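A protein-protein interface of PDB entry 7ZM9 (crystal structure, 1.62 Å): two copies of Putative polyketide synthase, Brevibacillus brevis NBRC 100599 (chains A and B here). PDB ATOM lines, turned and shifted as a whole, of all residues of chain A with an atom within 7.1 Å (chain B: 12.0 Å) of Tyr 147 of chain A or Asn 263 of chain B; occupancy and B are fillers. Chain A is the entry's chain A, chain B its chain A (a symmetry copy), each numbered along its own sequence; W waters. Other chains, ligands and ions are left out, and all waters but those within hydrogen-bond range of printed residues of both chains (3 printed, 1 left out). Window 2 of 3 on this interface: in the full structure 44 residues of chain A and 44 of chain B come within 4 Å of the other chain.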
ATOM      1  N   PHE A  80      -6.815 -18.547   5.162  1.00  0.00           N
ATOM      2  CA  PHE A  80      -6.655 -17.331   4.389  1.00  0.00           C
ATOM      3  C   PHE A  80      -7.936 -16.940   3.671  1.00  0.00           C
ATOM      4  O   PHE A  80      -7.927 -16.023   2.851  1.00  0.00           O
ATOM      5  CB  PHE A  80      -5.511 -17.511   3.389  1.00  0.00           C
ATOM      6  CG  PHE A  80      -4.185 -17.772   4.035  1.00  0.00           C
ATOM      7  CD1 PHE A  80      -3.429 -16.722   4.546  1.00  0.00           C
ATOM      8  CD2 PHE A  80      -3.670 -19.052   4.119  1.00  0.00           C
ATOM      9  CE1 PHE A  80      -2.207 -16.960   5.130  1.00  0.00           C
ATOM     10  CE2 PHE A  80      -2.461 -19.287   4.717  1.00  0.00           C
ATOM     11  CZ  PHE A  80      -1.727 -18.244   5.211  1.00  0.00           C
ATOM     12  N   ALA A 142       4.393 -13.359  -4.803  1.00  0.00           N
ATOM     13  CA  ALA A 142       4.590 -12.173  -3.981  1.00  0.00           C
ATOM     14  C   ALA A 142       3.274 -11.466  -3.670  1.00  0.00           C
ATOM     15  O   ALA A 142       3.047 -11.039  -2.527  1.00  0.00           O
ATOM     16  CB  ALA A 142       5.518 -11.169  -4.676  1.00  0.00           C
ATOM     17  N   ASN A 143       2.419 -11.289  -4.690  1.00  0.00           N
ATOM     18  CA  ASN A 143       1.269 -10.420  -4.528  1.00  0.00           C
ATOM     19  C   ASN A 143       0.204 -11.014  -3.621  1.00  0.00           C
ATOM     20  O   ASN A 143      -0.537 -10.257  -2.975  1.00  0.00           O
ATOM     21  CB  ASN A 143       0.627 -10.101  -5.888  1.00  0.00           C
ATOM     22  CG  ASN A 143       1.536  -9.256  -6.777  1.00  0.00           C
ATOM     23  OD1 ASN A 143       2.527  -8.637  -6.329  1.00  0.00           O
ATOM     24  ND2 ASN A 143       1.208  -9.204  -7.987  1.00  0.00           N
ATOM     25  N   ARG A 144       0.090 -12.341  -3.559  1.00  0.00           N
ATOM     26  CA  ARG A 144      -0.907 -12.945  -2.674  1.00  0.00           C
ATOM     27  C   ARG A 144      -0.598 -12.587  -1.234  1.00  0.00           C
ATOM     28  O   ARG A 144      -1.499 -12.290  -0.441  1.00  0.00           O
ATOM     29  CB  ARG A 144      -0.898 -14.465  -2.848  1.00  0.00           C
ATOM     30  CG  ARG A 144      -1.888 -15.243  -2.004  1.00  0.00           C
ATOM     31  CD  ARG A 144      -3.294 -15.236  -2.617  1.00  0.00           C
ATOM     32  NE  ARG A 144      -3.345 -15.901  -3.915  1.00  0.00           N
ATOM     33  CZ  ARG A 144      -4.460 -16.180  -4.577  1.00  0.00           C
ATOM     34  NH1 ARG A 144      -5.633 -15.857  -4.057  1.00  0.00           N
ATOM     35  NH2 ARG A 144      -4.401 -16.763  -5.769  1.00  0.00           N
ATOM     36  N   LEU A 145       0.687 -12.621  -0.885  1.00  0.00           N
ATOM     37  CA  LEU A 145       1.110 -12.258   0.460  1.00  0.00           C
ATOM     38  C   LEU A 145       0.782 -10.795   0.732  1.00  0.00           C
ATOM     39  O   LEU A 145       0.181 -10.461   1.759  1.00  0.00           O
ATOM     40  CB  LEU A 145       2.602 -12.518   0.612  1.00  0.00           C
ATOM     41  CG  LEU A 145       3.168 -12.222   2.004  1.00  0.00           C
ATOM     42  CD1 LEU A 145       2.600 -13.107   3.075  1.00  0.00           C
ATOM     43  CD2 LEU A 145       4.675 -12.316   1.945  1.00  0.00           C
ATOM     44  N   SER A 146       1.152  -9.914  -0.193  1.00  0.00           N
ATOM     45  CA  SER A 146       0.924  -8.492   0.025  1.00  0.00           C
ATOM     46  C   SER A 146      -0.560  -8.188   0.158  1.00  0.00           C
ATOM     47  O   SER A 146      -0.965  -7.359   0.972  1.00  0.00           O
ATOM     48  CB  SER A 146       1.522  -7.694  -1.121  1.00  0.00           C
ATOM     49  OG  SER A 146       2.908  -7.799  -1.145  1.00  0.00           O
ATOM     50  N   TYR A 147      -1.392  -8.845  -0.654  1.00  0.00           N
ATOM     51  CA  TYR A 147      -2.832  -8.657  -0.551  1.00  0.00           C
ATOM     52  C   TYR A 147      -3.359  -9.131   0.799  1.00  0.00           C
ATOM     53  O   TYR A 147      -4.038  -8.382   1.513  1.00  0.00           O
ATOM     54  CB  TYR A 147      -3.538  -9.407  -1.690  1.00  0.00           C
ATOM     55  CG  TYR A 147      -5.027  -9.523  -1.471  1.00  0.00           C
ATOM     56  CD1 TYR A 147      -5.876  -8.449  -1.744  1.00  0.00           C
ATOM     57  CD2 TYR A 147      -5.590 -10.689  -0.983  1.00  0.00           C
ATOM     58  CE1 TYR A 147      -7.226  -8.561  -1.524  1.00  0.00           C
ATOM     59  CE2 TYR A 147      -6.958 -10.804  -0.774  1.00  0.00           C
ATOM     60  CZ  TYR A 147      -7.757  -9.727  -1.049  1.00  0.00           C
ATOM     61  OH  TYR A 147      -9.110  -9.795  -0.836  1.00  0.00           O
ATOM     62  N   LEU A 148      -3.065 -10.381   1.171  1.00  0.00           N
ATOM     63  CA  LEU A 148      -3.721 -10.942   2.340  1.00  0.00           C
ATOM     64  C   LEU A 148      -3.311 -10.237   3.617  1.00  0.00           C
ATOM     65  O   LEU A 148      -4.133 -10.067   4.526  1.00  0.00           O
ATOM     66  CB  LEU A 148      -3.423 -12.429   2.444  1.00  0.00           C
ATOM     67  CG  LEU A 148      -4.162 -13.295   1.424  1.00  0.00           C
ATOM     68  CD1 LEU A 148      -3.530 -14.698   1.410  1.00  0.00           C
ATOM     69  CD2 LEU A 148      -5.646 -13.367   1.697  1.00  0.00           C
ATOM     70  N   LEU A 149      -2.053  -9.805   3.706  1.00  0.00           N
ATOM     71  CA  LEU A 149      -1.513  -9.201   4.917  1.00  0.00           C
ATOM     72  C   LEU A 149      -1.489  -7.687   4.860  1.00  0.00           C
ATOM     73  O   LEU A 149      -0.971  -7.050   5.766  1.00  0.00           O
ATOM     74  CB  LEU A 149      -0.113  -9.752   5.170  1.00  0.00           C
ATOM     75  CG  LEU A 149      -0.144 -11.088   5.904  1.00  0.00           C
ATOM     76  CD1 LEU A 149      -0.862 -12.131   5.198  1.00  0.00           C
ATOM     77  CD2 LEU A 149       1.308 -11.548   6.273  1.00  0.00           C
ATOM     78  N   ASN A 150      -2.105  -7.101   3.845  1.00  0.00           N
ATOM     79  CA  ASN A 150      -2.186  -5.660   3.680  1.00  0.00           C
ATOM     80  C   ASN A 150      -0.813  -4.999   3.681  1.00  0.00           C
ATOM     81  O   ASN A 150      -0.582  -4.006   4.371  1.00  0.00           O
ATOM     82  CB  ASN A 150      -3.090  -5.025   4.741  1.00  0.00           C
ATOM     83  CG  ASN A 150      -3.435  -3.593   4.401  1.00  0.00           C
ATOM     84  OD1 ASN A 150      -3.533  -3.241   3.229  1.00  0.00           O
ATOM     85  ND2 ASN A 150      -3.597  -2.762   5.409  1.00  0.00           N
ATOM     86  N   PHE A 151       0.090  -5.541   2.874  1.00  0.00           N
ATOM     87  CA  PHE A 151       1.401  -4.925   2.654  1.00  0.00           C
ATOM     88  C   PHE A 151       1.335  -4.052   1.401  1.00  0.00           C
ATOM     89  O   PHE A 151       0.802  -4.471   0.360  1.00  0.00           O
ATOM     90  CB  PHE A 151       2.491  -5.973   2.474  1.00  0.00           C
ATOM     91  CG  PHE A 151       2.719  -6.847   3.687  1.00  0.00           C
ATOM     92  CD1 PHE A 151       2.374  -6.413   4.955  1.00  0.00           C
ATOM     93  CD2 PHE A 151       3.305  -8.105   3.541  1.00  0.00           C
ATOM     94  CE1 PHE A 151       2.648  -7.215   6.079  1.00  0.00           C
ATOM     95  CE2 PHE A 151       3.528  -8.898   4.618  1.00  0.00           C
ATOM     96  CZ  PHE A 151       3.212  -8.445   5.902  1.00  0.00           C
ATOM     97  N   SER A 155       6.216  -5.220  -4.229  1.00  0.00           N
ATOM     98  CA  SER A 155       5.845  -6.640  -4.197  1.00  0.00           C
ATOM     99  C   SER A 155       6.232  -7.243  -5.533  1.00  0.00           C
ATOM    100  O   SER A 155       5.635  -6.885  -6.571  1.00  0.00           O
ATOM    101  CB  SER A 155       4.351  -6.780  -3.921  1.00  0.00           C
ATOM    102  OG  SER A 155       3.932  -8.102  -3.709  1.00  0.00           O
ATOM    103  N   ASN B 257       4.980   0.245  -5.450  1.00  0.00           N
ATOM    104  CA  ASN B 257       4.273  -0.079  -4.225  1.00  0.00           C
ATOM    105  C   ASN B 257       3.242  -1.159  -4.545  1.00  0.00           C
ATOM    106  O   ASN B 257       3.282  -1.766  -5.608  1.00  0.00           O
ATOM    107  CB  ASN B 257       3.688   1.181  -3.560  1.00  0.00           C
ATOM    108  CG  ASN B 257       2.310   1.559  -4.057  1.00  0.00           C
ATOM    109  OD1 ASN B 257       1.877   1.097  -5.077  1.00  0.00           O
ATOM    110  ND2 ASN B 257       1.648   2.405  -3.307  1.00  0.00           N
ATOM    111  N   ALA B 258       2.404  -1.485  -3.570  1.00  0.00           N
ATOM    112  CA  ALA B 258       1.385  -2.509  -3.781  1.00  0.00           C
ATOM    113  C   ALA B 258       0.088  -2.064  -3.122  1.00  0.00           C
ATOM    114  O   ALA B 258       0.058  -1.228  -2.218  1.00  0.00           O
ATOM    115  CB  ALA B 258       1.806  -3.892  -3.240  1.00  0.00           C
ATOM    116  N   GLY B 259      -1.006  -2.651  -3.581  1.00  0.00           N
ATOM    117  CA  GLY B 259      -2.305  -2.202  -3.089  1.00  0.00           C
ATOM    118  C   GLY B 259      -2.701  -2.747  -1.753  1.00  0.00           C
ATOM    119  O   GLY B 259      -3.635  -2.243  -1.132  1.00  0.00           O
ATOM    120  N   GLY B 260      -2.012  -3.766  -1.262  1.00  0.00           N
ATOM    121  CA  GLY B 260      -2.461  -4.303   0.004  1.00  0.00           C
ATOM    122  C   GLY B 260      -3.830  -4.946  -0.083  1.00  0.00           C
ATOM    123  O   GLY B 260      -4.224  -5.498  -1.102  1.00  0.00           O
ATOM    124  N   LYS B 261      -4.545  -4.895   1.023  1.00  0.00           N
ATOM    125  CA  LYS B 261      -5.804  -5.610   1.156  1.00  0.00           C
ATOM    126  C   LYS B 261      -6.927  -4.738   0.601  1.00  0.00           C
ATOM    127  O   LYS B 261      -7.173  -3.637   1.101  1.00  0.00           O
ATOM    128  CB  LYS B 261      -6.090  -5.966   2.606  1.00  0.00           C
ATOM    129  CG  LYS B 261      -7.382  -6.793   2.829  1.00  0.00           C
ATOM    130  CD  LYS B 261      -7.265  -8.211   2.249  1.00  0.00           C
ATOM    131  CE  LYS B 261      -8.447  -9.090   2.629  1.00  0.00           C
ATOM    132  NZ  LYS B 261      -9.672  -8.601   1.951  1.00  0.00           N
ATOM    133  N   THR B 262      -7.561  -5.219  -0.448  1.00  0.00           N
ATOM    134  CA  THR B 262      -8.769  -4.651  -1.035  1.00  0.00           C
ATOM    135  C   THR B 262      -9.905  -5.662  -0.884  1.00  0.00           C
ATOM    136  O   THR B 262      -9.761  -6.716  -0.245  1.00  0.00           O
ATOM    137  CB  THR B 262      -8.493  -4.295  -2.490  1.00  0.00           C
ATOM    138  OG1 THR B 262      -7.990  -5.457  -3.160  1.00  0.00           O
ATOM    139  CG2 THR B 262      -7.425  -3.222  -2.593  1.00  0.00           C
ATOM    140  N   ASN B 263     -11.054  -5.347  -1.490  1.00  0.00           N
ATOM    141  CA  ASN B 263     -12.241  -6.149  -1.239  1.00  0.00           C
ATOM    142  C   ASN B 263     -12.118  -7.554  -1.800  1.00  0.00           C
ATOM    143  O   ASN B 263     -12.834  -8.452  -1.353  1.00  0.00           O
ATOM    144  CB  ASN B 263     -13.490  -5.454  -1.812  1.00  0.00           C
ATOM    145  CG  ASN B 263     -14.758  -6.205  -1.477  1.00  0.00           C
ATOM    146  OD1 ASN B 263     -14.767  -7.037  -0.564  1.00  0.00           O
ATOM    147  ND2 ASN B 263     -15.832  -5.932  -2.213  1.00  0.00           N
ATOM    148  N   GLY B 264     -11.200  -7.768  -2.726  1.00  0.00           N
ATOM    149  CA  GLY B 264     -10.914  -9.098  -3.215  1.00  0.00           C
ATOM    150  C   GLY B 264      -9.596  -9.055  -3.948  1.00  0.00           C
ATOM    151  O   GLY B 264      -9.135  -7.989  -4.374  1.00  0.00           O
ATOM    152  N   TYR B 265      -8.967 -10.225  -4.043  1.00  0.00           N
ATOM    153  CA  TYR B 265      -7.653 -10.291  -4.673  1.00  0.00           C
ATOM    154  C   TYR B 265      -7.760  -9.797  -6.099  1.00  0.00           C
ATOM    155  O   TYR B 265      -8.682 -10.205  -6.823  1.00  0.00           O
ATOM    156  CB  TYR B 265      -7.127 -11.712  -4.645  1.00  0.00           C
ATOM    157  CG  TYR B 265      -5.694 -11.882  -5.115  1.00  0.00           C
ATOM    158  CD1 TYR B 265      -4.678 -11.061  -4.642  1.00  0.00           C
ATOM    159  CD2 TYR B 265      -5.340 -12.908  -5.972  1.00  0.00           C
ATOM    160  CE1 TYR B 265      -3.358 -11.261  -5.056  1.00  0.00           C
ATOM    161  CE2 TYR B 265      -4.057 -13.104  -6.399  1.00  0.00           C
ATOM    162  CZ  TYR B 265      -3.051 -12.300  -5.889  1.00  0.00           C
ATOM    163  OH  TYR B 265      -1.786 -12.488  -6.335  1.00  0.00           O
ATOM    164  N   THR B 266      -6.803  -8.959  -6.503  1.00  0.00           N
ATOM    165  CA  THR B 266      -6.736  -8.254  -7.800  1.00  0.00           C
ATOM    166  C   THR B 266      -7.680  -7.055  -7.936  1.00  0.00           C
ATOM    167  O   THR B 266      -7.754  -6.474  -9.028  1.00  0.00           O
ATOM    168  CB  THR B 266      -6.974  -9.173  -9.022  1.00  0.00           C
ATOM    169  OG1 THR B 266      -8.363  -9.515  -9.150  1.00  0.00           O
ATOM    170  CG2 THR B 266      -6.103 -10.451  -8.896  1.00  0.00           C
ATOM    171  N   VAL B 267      -8.402  -6.666  -6.892  1.00  0.00           N
ATOM    172  CA  VAL B 267      -9.144  -5.414  -6.933  1.00  0.00           C
ATOM    173  C   VAL B 267      -8.146  -4.279  -6.682  1.00  0.00           C
ATOM    174  O   VAL B 267      -7.426  -4.311  -5.672  1.00  0.00           O
ATOM    175  CB  VAL B 267     -10.281  -5.405  -5.900  1.00  0.00           C
ATOM    176  CG1 VAL B 267     -10.924  -4.050  -5.850  1.00  0.00           C
ATOM    177  CG2 VAL B 267     -11.309  -6.473  -6.237  1.00  0.00           C
ATOM    178  N   PRO B 268      -8.056  -3.272  -7.557  1.00  0.00           N
ATOM    179  CA  PRO B 268      -7.101  -2.171  -7.335  1.00  0.00           C
ATOM    180  C   PRO B 268      -7.506  -1.248  -6.193  1.00  0.00           C
ATOM    181  O   PRO B 268      -8.663  -1.140  -5.821  1.00  0.00           O
ATOM    182  CB  PRO B 268      -7.081  -1.433  -8.678  1.00  0.00           C
ATOM    183  CG  PRO B 268      -8.409  -1.798  -9.315  1.00  0.00           C
ATOM    184  CD  PRO B 268      -8.802  -3.133  -8.826  1.00  0.00           C
ATOM    185  N   ASN B 269      -6.495  -0.594  -5.598  1.00  0.00           N
ATOM    186  CA  ASN B 269      -6.699   0.241  -4.421  1.00  0.00           C
ATOM    187  C   ASN B 269      -6.424   1.707  -4.747  1.00  0.00           C
ATOM    188  O   ASN B 269      -5.259   2.075  -4.953  1.00  0.00           O
ATOM    189  CB  ASN B 269      -5.738  -0.233  -3.316  1.00  0.00           C
ATOM    190  CG  ASN B 269      -5.944   0.487  -2.019  1.00  0.00           C
ATOM    191  OD1 ASN B 269      -6.591   1.522  -1.971  1.00  0.00           O
ATOM    192  ND2 ASN B 269      -5.420  -0.066  -0.954  1.00  0.00           N
ATOM    193  N   PRO B 270      -7.424   2.587  -4.788  1.00  0.00           N
ATOM    194  CA  PRO B 270      -7.127   3.981  -5.137  1.00  0.00           C
ATOM    195  C   PRO B 270      -6.261   4.690  -4.123  1.00  0.00           C
ATOM    196  O   PRO B 270      -5.500   5.575  -4.504  1.00  0.00           O
ATOM    197  CB  PRO B 270      -8.518   4.636  -5.207  1.00  0.00           C
ATOM    198  CG  PRO B 270      -9.397   3.765  -4.320  1.00  0.00           C
ATOM    199  CD  PRO B 270      -8.847   2.368  -4.454  1.00  0.00           C
ATOM    200  N   GLN B 271      -6.369   4.336  -2.840  1.00  0.00           N
ATOM    201  CA  GLN B 271      -5.523   4.948  -1.814  1.00  0.00           C
ATOM    202  C   GLN B 271      -4.051   4.608  -2.039  1.00  0.00           C
ATOM    203  O   GLN B 271      -3.173   5.473  -1.907  1.00  0.00           O
ATOM    204  CB  GLN B 271      -5.997   4.476  -0.426  1.00  0.00           C
ATOM    205  CG  GLN B 271      -5.006   4.660   0.763  1.00  0.00           C
ATOM    206  CD  GLN B 271      -4.069   3.416   1.033  1.00  0.00           C
ATOM    207  OE1 GLN B 271      -4.521   2.277   1.190  1.00  0.00           O
ATOM    208  NE2 GLN B 271      -2.760   3.665   1.089  1.00  0.00           N
ATOM    209  N   ALA B 272      -3.755   3.350  -2.383  1.00  0.00           N
ATOM    210  CA  ALA B 272      -2.379   2.965  -2.651  1.00  0.00           C
ATOM    211  C   ALA B 272      -1.860   3.566  -3.943  1.00  0.00           C
ATOM    212  O   ALA B 272      -0.680   3.931  -4.027  1.00  0.00           O
ATOM    213  CB  ALA B 272      -2.261   1.437  -2.695  1.00  0.00           C
ATOM    214  N   GLN B 273      -2.721   3.675  -4.979  1.00  0.00           N
ATOM    215  CA  GLN B 273      -2.284   4.345  -6.201  1.00  0.00           C
ATOM    216  C   GLN B 273      -1.952   5.801  -5.921  1.00  0.00           C
ATOM    217  O   GLN B 273      -0.982   6.336  -6.468  1.00  0.00           O
ATOM    218  CB  GLN B 273      -3.372   4.256  -7.291  1.00  0.00           C
ATOM    219  CG  GLN B 273      -3.606   2.834  -7.755  1.00  0.00           C
ATOM    220  CD  GLN B 273      -4.742   2.739  -8.745  1.00  0.00           C
ATOM    221  OE1 GLN B 273      -5.338   3.751  -9.106  1.00  0.00           O
ATOM    222  NE2 GLN B 273      -5.055   1.532  -9.188  1.00  0.00           N
ATOM    223  N   LEU B 303     -14.420  -1.190 -13.451  1.00  0.00           N
ATOM    224  CA  LEU B 303     -13.925  -1.068 -12.084  1.00  0.00           C
ATOM    225  C   LEU B 303     -12.670  -0.205 -12.030  1.00  0.00           C
ATOM    226  O   LEU B 303     -12.557   0.697 -11.190  1.00  0.00           O
ATOM    227  CB  LEU B 303     -13.609  -2.463 -11.514  1.00  0.00           C
ATOM    228  CG  LEU B 303     -12.938  -2.567 -10.138  1.00  0.00           C
ATOM    229  CD1 LEU B 303     -13.880  -2.121  -9.029  1.00  0.00           C
ATOM    230  CD2 LEU B 303     -12.451  -3.970  -9.869  1.00  0.00           C
ATOM    231  N   ILE B 307     -11.262   4.092 -10.474  1.00  0.00           N
ATOM    232  CA  ILE B 307     -10.286   3.980  -9.391  1.00  0.00           C
ATOM    233  C   ILE B 307      -9.014   4.711  -9.759  1.00  0.00           C
ATOM    234  O   ILE B 307      -8.417   5.408  -8.927  1.00  0.00           O
ATOM    235  CB  ILE B 307     -10.044   2.491  -9.071  1.00  0.00           C
ATOM    236  CG1 ILE B 307     -11.235   2.002  -8.229  1.00  0.00           C
ATOM    237  CG2 ILE B 307      -8.706   2.276  -8.361  1.00  0.00           C
ATOM    238  CD1 ILE B 307     -11.269   0.504  -8.004  1.00  0.00           C
ATOM    239  N   GLY B 412      -0.252  -3.801 -11.952  1.00  0.00           N
ATOM    240  CA  GLY B 412      -0.412  -5.198 -12.221  1.00  0.00           C
ATOM    241  C   GLY B 412      -1.660  -5.742 -11.577  1.00  0.00           C
ATOM    242  O   GLY B 412      -2.112  -5.254 -10.562  1.00  0.00           O
ATOM    243  N   ALA B 413      -2.174  -6.819 -12.173  1.00  0.00           N
ATOM    244  CA  ALA B 413      -3.402  -7.418 -11.691  1.00  0.00           C
ATOM    245  C   ALA B 413      -3.314  -7.810 -10.226  1.00  0.00           C
ATOM    246  O   ALA B 413      -4.310  -7.732  -9.505  1.00  0.00           O
ATOM    247  CB  ALA B 413      -3.746  -8.626 -12.559  1.00  0.00           C
ATOM    248  N   GLY B 414      -2.142  -8.290  -9.768  1.00  0.00           N
ATOM    249  CA  GLY B 414      -2.025  -8.704  -8.385  1.00  0.00           C
ATOM    250  C   GLY B 414      -1.820  -7.573  -7.403  1.00  0.00           C
ATOM    251  O   GLY B 414      -1.790  -7.818  -6.200  1.00  0.00           O
ATOM    252  N   GLY B 415      -1.765  -6.343  -7.907  1.00  0.00           N
ATOM    253  CA  GLY B 415      -1.675  -5.162  -7.079  1.00  0.00           C
ATOM    254  C   GLY B 415      -0.318  -4.488  -7.011  1.00  0.00           C
ATOM    255  O   GLY B 415      -0.150  -3.559  -6.196  1.00  0.00           O
ATOM    256  N   SER B 416       0.664  -4.934  -7.800  1.00  0.00           N
ATOM    257  CA  SER B 416       1.960  -4.261  -7.819  1.00  0.00           C
ATOM    258  C   SER B 416       1.905  -3.077  -8.751  1.00  0.00           C
ATOM    259  O   SER B 416       1.571  -3.240  -9.934  1.00  0.00           O
ATOM    260  CB  SER B 416       3.097  -5.154  -8.311  1.00  0.00           C
ATOM    261  OG  SER B 416       3.283  -6.228  -7.465  1.00  0.00           O
ATOM    262  N   ASN B 417       2.230  -1.901  -8.236  1.00  0.00           N
ATOM    263  CA  ASN B 417       2.073  -0.656  -8.963  1.00  0.00           C
ATOM    264  C   ASN B 417       3.411  -0.002  -9.173  1.00  0.00           C
ATOM    265  O   ASN B 417       4.317  -0.162  -8.342  1.00  0.00           O
ATOM    266  CB  ASN B 417       1.202   0.283  -8.154  1.00  0.00           C
ATOM    267  CG  ASN B 417      -0.110  -0.334  -7.790  1.00  0.00           C
ATOM    268  OD1 ASN B 417      -0.788  -0.957  -8.638  1.00  0.00           O
ATOM    269  ND2 ASN B 417      -0.521  -0.134  -6.534  1.00  0.00           N
HETATM  270  O   HOH W   1       5.348  -3.442  -6.385  1.00  0.00           O
HETATM  271  O   HOH W   2      -0.952  -7.254  -3.797  1.00  0.00           O
HETATM  272  O   HOH W   3      -5.682  -1.641   2.279  1.00  0.00           O
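The side-chain amide oxygen (OD1) of Asn 143 of chain A sits at hydrogen-bond distance from the side-chain hydroxyl (OG) of Ser 416 of chain B, 2.8 Å away.
The side-chain hydroxyl (OH) of Tyr 265 of chain B sits at hydrogen-bond distance from the backbone NH (N) of Arg 144 of chain A, 3.4 Å away.
The side-chain hydroxyl (OH) of Tyr 147 of chain A sits at hydrogen-bond distance from the side-chain amino group (NZ) of Lys 261 of chain B.
OH of Tyr 147 of chain A is in hydrogen-bond range of O of Thr 262 of chain B (3.2 Å).
N of Gly 264 of chain B sits close to OH of Tyr 147 of chain A, at 3.5 Å.
The side-chain hydroxyl (OH) of Tyr 147 of chain A lies within hydrogen-bond range of the backbone NH (N) of Tyr 265 of chain B (3.2 Å).
The backbone NH (N) of Lys 261 of chain B sits at hydrogen-bond distance from the side-chain amide oxygen (OD1) of Asn 150 of chain A (2.9 Å).
The backbone NH (N) of Gly 260 of chain B lies close to the backbone carbonyl oxygen (O) of Phe 151 of chain A (3.3 Å).
O of Ser 155 of chain A is in hydrogen-bond range of OG of Ser 416 of chain B (2.6 Å).
OG of Ser 155 of chain A is in hydrogen-bond range of O of Ala 142 of chain A, at 3.3 Å.
The side-chain hydroxyl of Ser 155 of chain A sits at hydrogen-bond distance from the side-chain amide oxygen of Asn 143 of chain A, 3.0 Å away.
O of Ser 146 of chain A lies within hydrogen-bond range of N of Phe 151 of chain A (2.8 Å).
The side-chain hydroxyl (OG) of Ser 155 of chain A is in hydrogen-bond range of the side-chain hydroxyl (OG) of Ser 146 of chain A (2.8 Å).
The backbone carbonyl oxygen (O) of Gly 264 of chain B is in hydrogen-bond range of the side-chain hydroxyl (OG1) of Thr 262 of chain B (3.0 Å).
The side-chain hydroxyl (OG1) of Thr 262 of chain B is in hydrogen-bond range of the backbone carbonyl oxygen (O) of Val 267 of chain B.
OH of Tyr 265 of chain B touches CB of Asn 143 of chain A, at 3.4 Å.
ND2 of Asn 143 of chain A touches CA of Gly 414 of chain B, 3.3 Å away.
CA of Gly 260 of chain B touches O of Ser 146 of chain A, at 3.5 Å.
Gly 260 of chain B touches Tyr 147 of chain A (O to CD1, 3.4 Å).
Tyr 147 of chain A touches Asn 263 of chain B.
Gly 260 of chain B touches Asn 150 of chain A.
Ala 258 of chain B touches Phe 151 of chain A.
Ala 258 of chain B touches Ser 155 of chain A (CB to CB, 3.9 Å).
Tyr 147 of chain A touches just these residues of chain B: Gly 260 (3.4 Å), Lys 261 (3.1 Å), Thr 262 (3.2 Å), Asn 263 (3.9 Å), Gly 264 (3.1 Å) and Tyr 265 (3.2 Å).
Asn 263 of chain B touches one residue of chain A.
Asn 143 of chain A touches just these residues of chain B: Tyr 265 (3.4 Å), Gly 414 (3.3 Å) and Ser 416 (2.8 Å).
Arg 144 of chain A touches just one residue of chain B: Tyr 265 (3.4 Å).
No residue of chain B comes within 4 Å of Leu 145 of chain A.
Ser 146 of chain A touches one residue of chain B.
No residue of chain B comes within 4 Å of Leu 148 of chain A.
Of the printed residues of chain A, Gly 414 of chain B touches Asn 143.
Of the printed residues of chain A, Lys 261 of chain B touches Tyr 147 (3.1 Å) and Asn 150 (2.9 Å).
Ile 307 of chain B touches none of the printed residues of chain A.
Asn 417 of chain B touches none of the printed residues of chain A.
The nearest printed residue of chain A that does not touch Asn 263 of chain B is Asn 150 of chain A (9.1 Å).
Hydrophobic or aromatic side chains of chain A within 4 Å of the printed part of chain B: Tyr 147.
Among the printed residues, 17 pairs touch across the chains.
Among the printed residues, no Asp or Glu carboxylate lies within 4 Å of a Lys or Arg side-chain nitrogen of the other chain.
No position is printed for both chains.
Of the 17 pairs that touch across the chains among the printed residues, none has its exchanged pair printed and touching as well.
Water W2 bridges O of Gly 414 of chain B (2.6 Å) and O of Asn 143 of chain A (3.1 Å).
Water W3 lies within hydrogen-bond range of the backbone carbonyl oxygen of Lys 261 of chain B (2.8 Å) and the side-chain amide oxygen of Asn 150 of chain A (2.8 Å).
Water W1 bridges O of Asn 257 of chain B (2.8 Å) and N of Ser 155 of chain A (2.9 Å).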
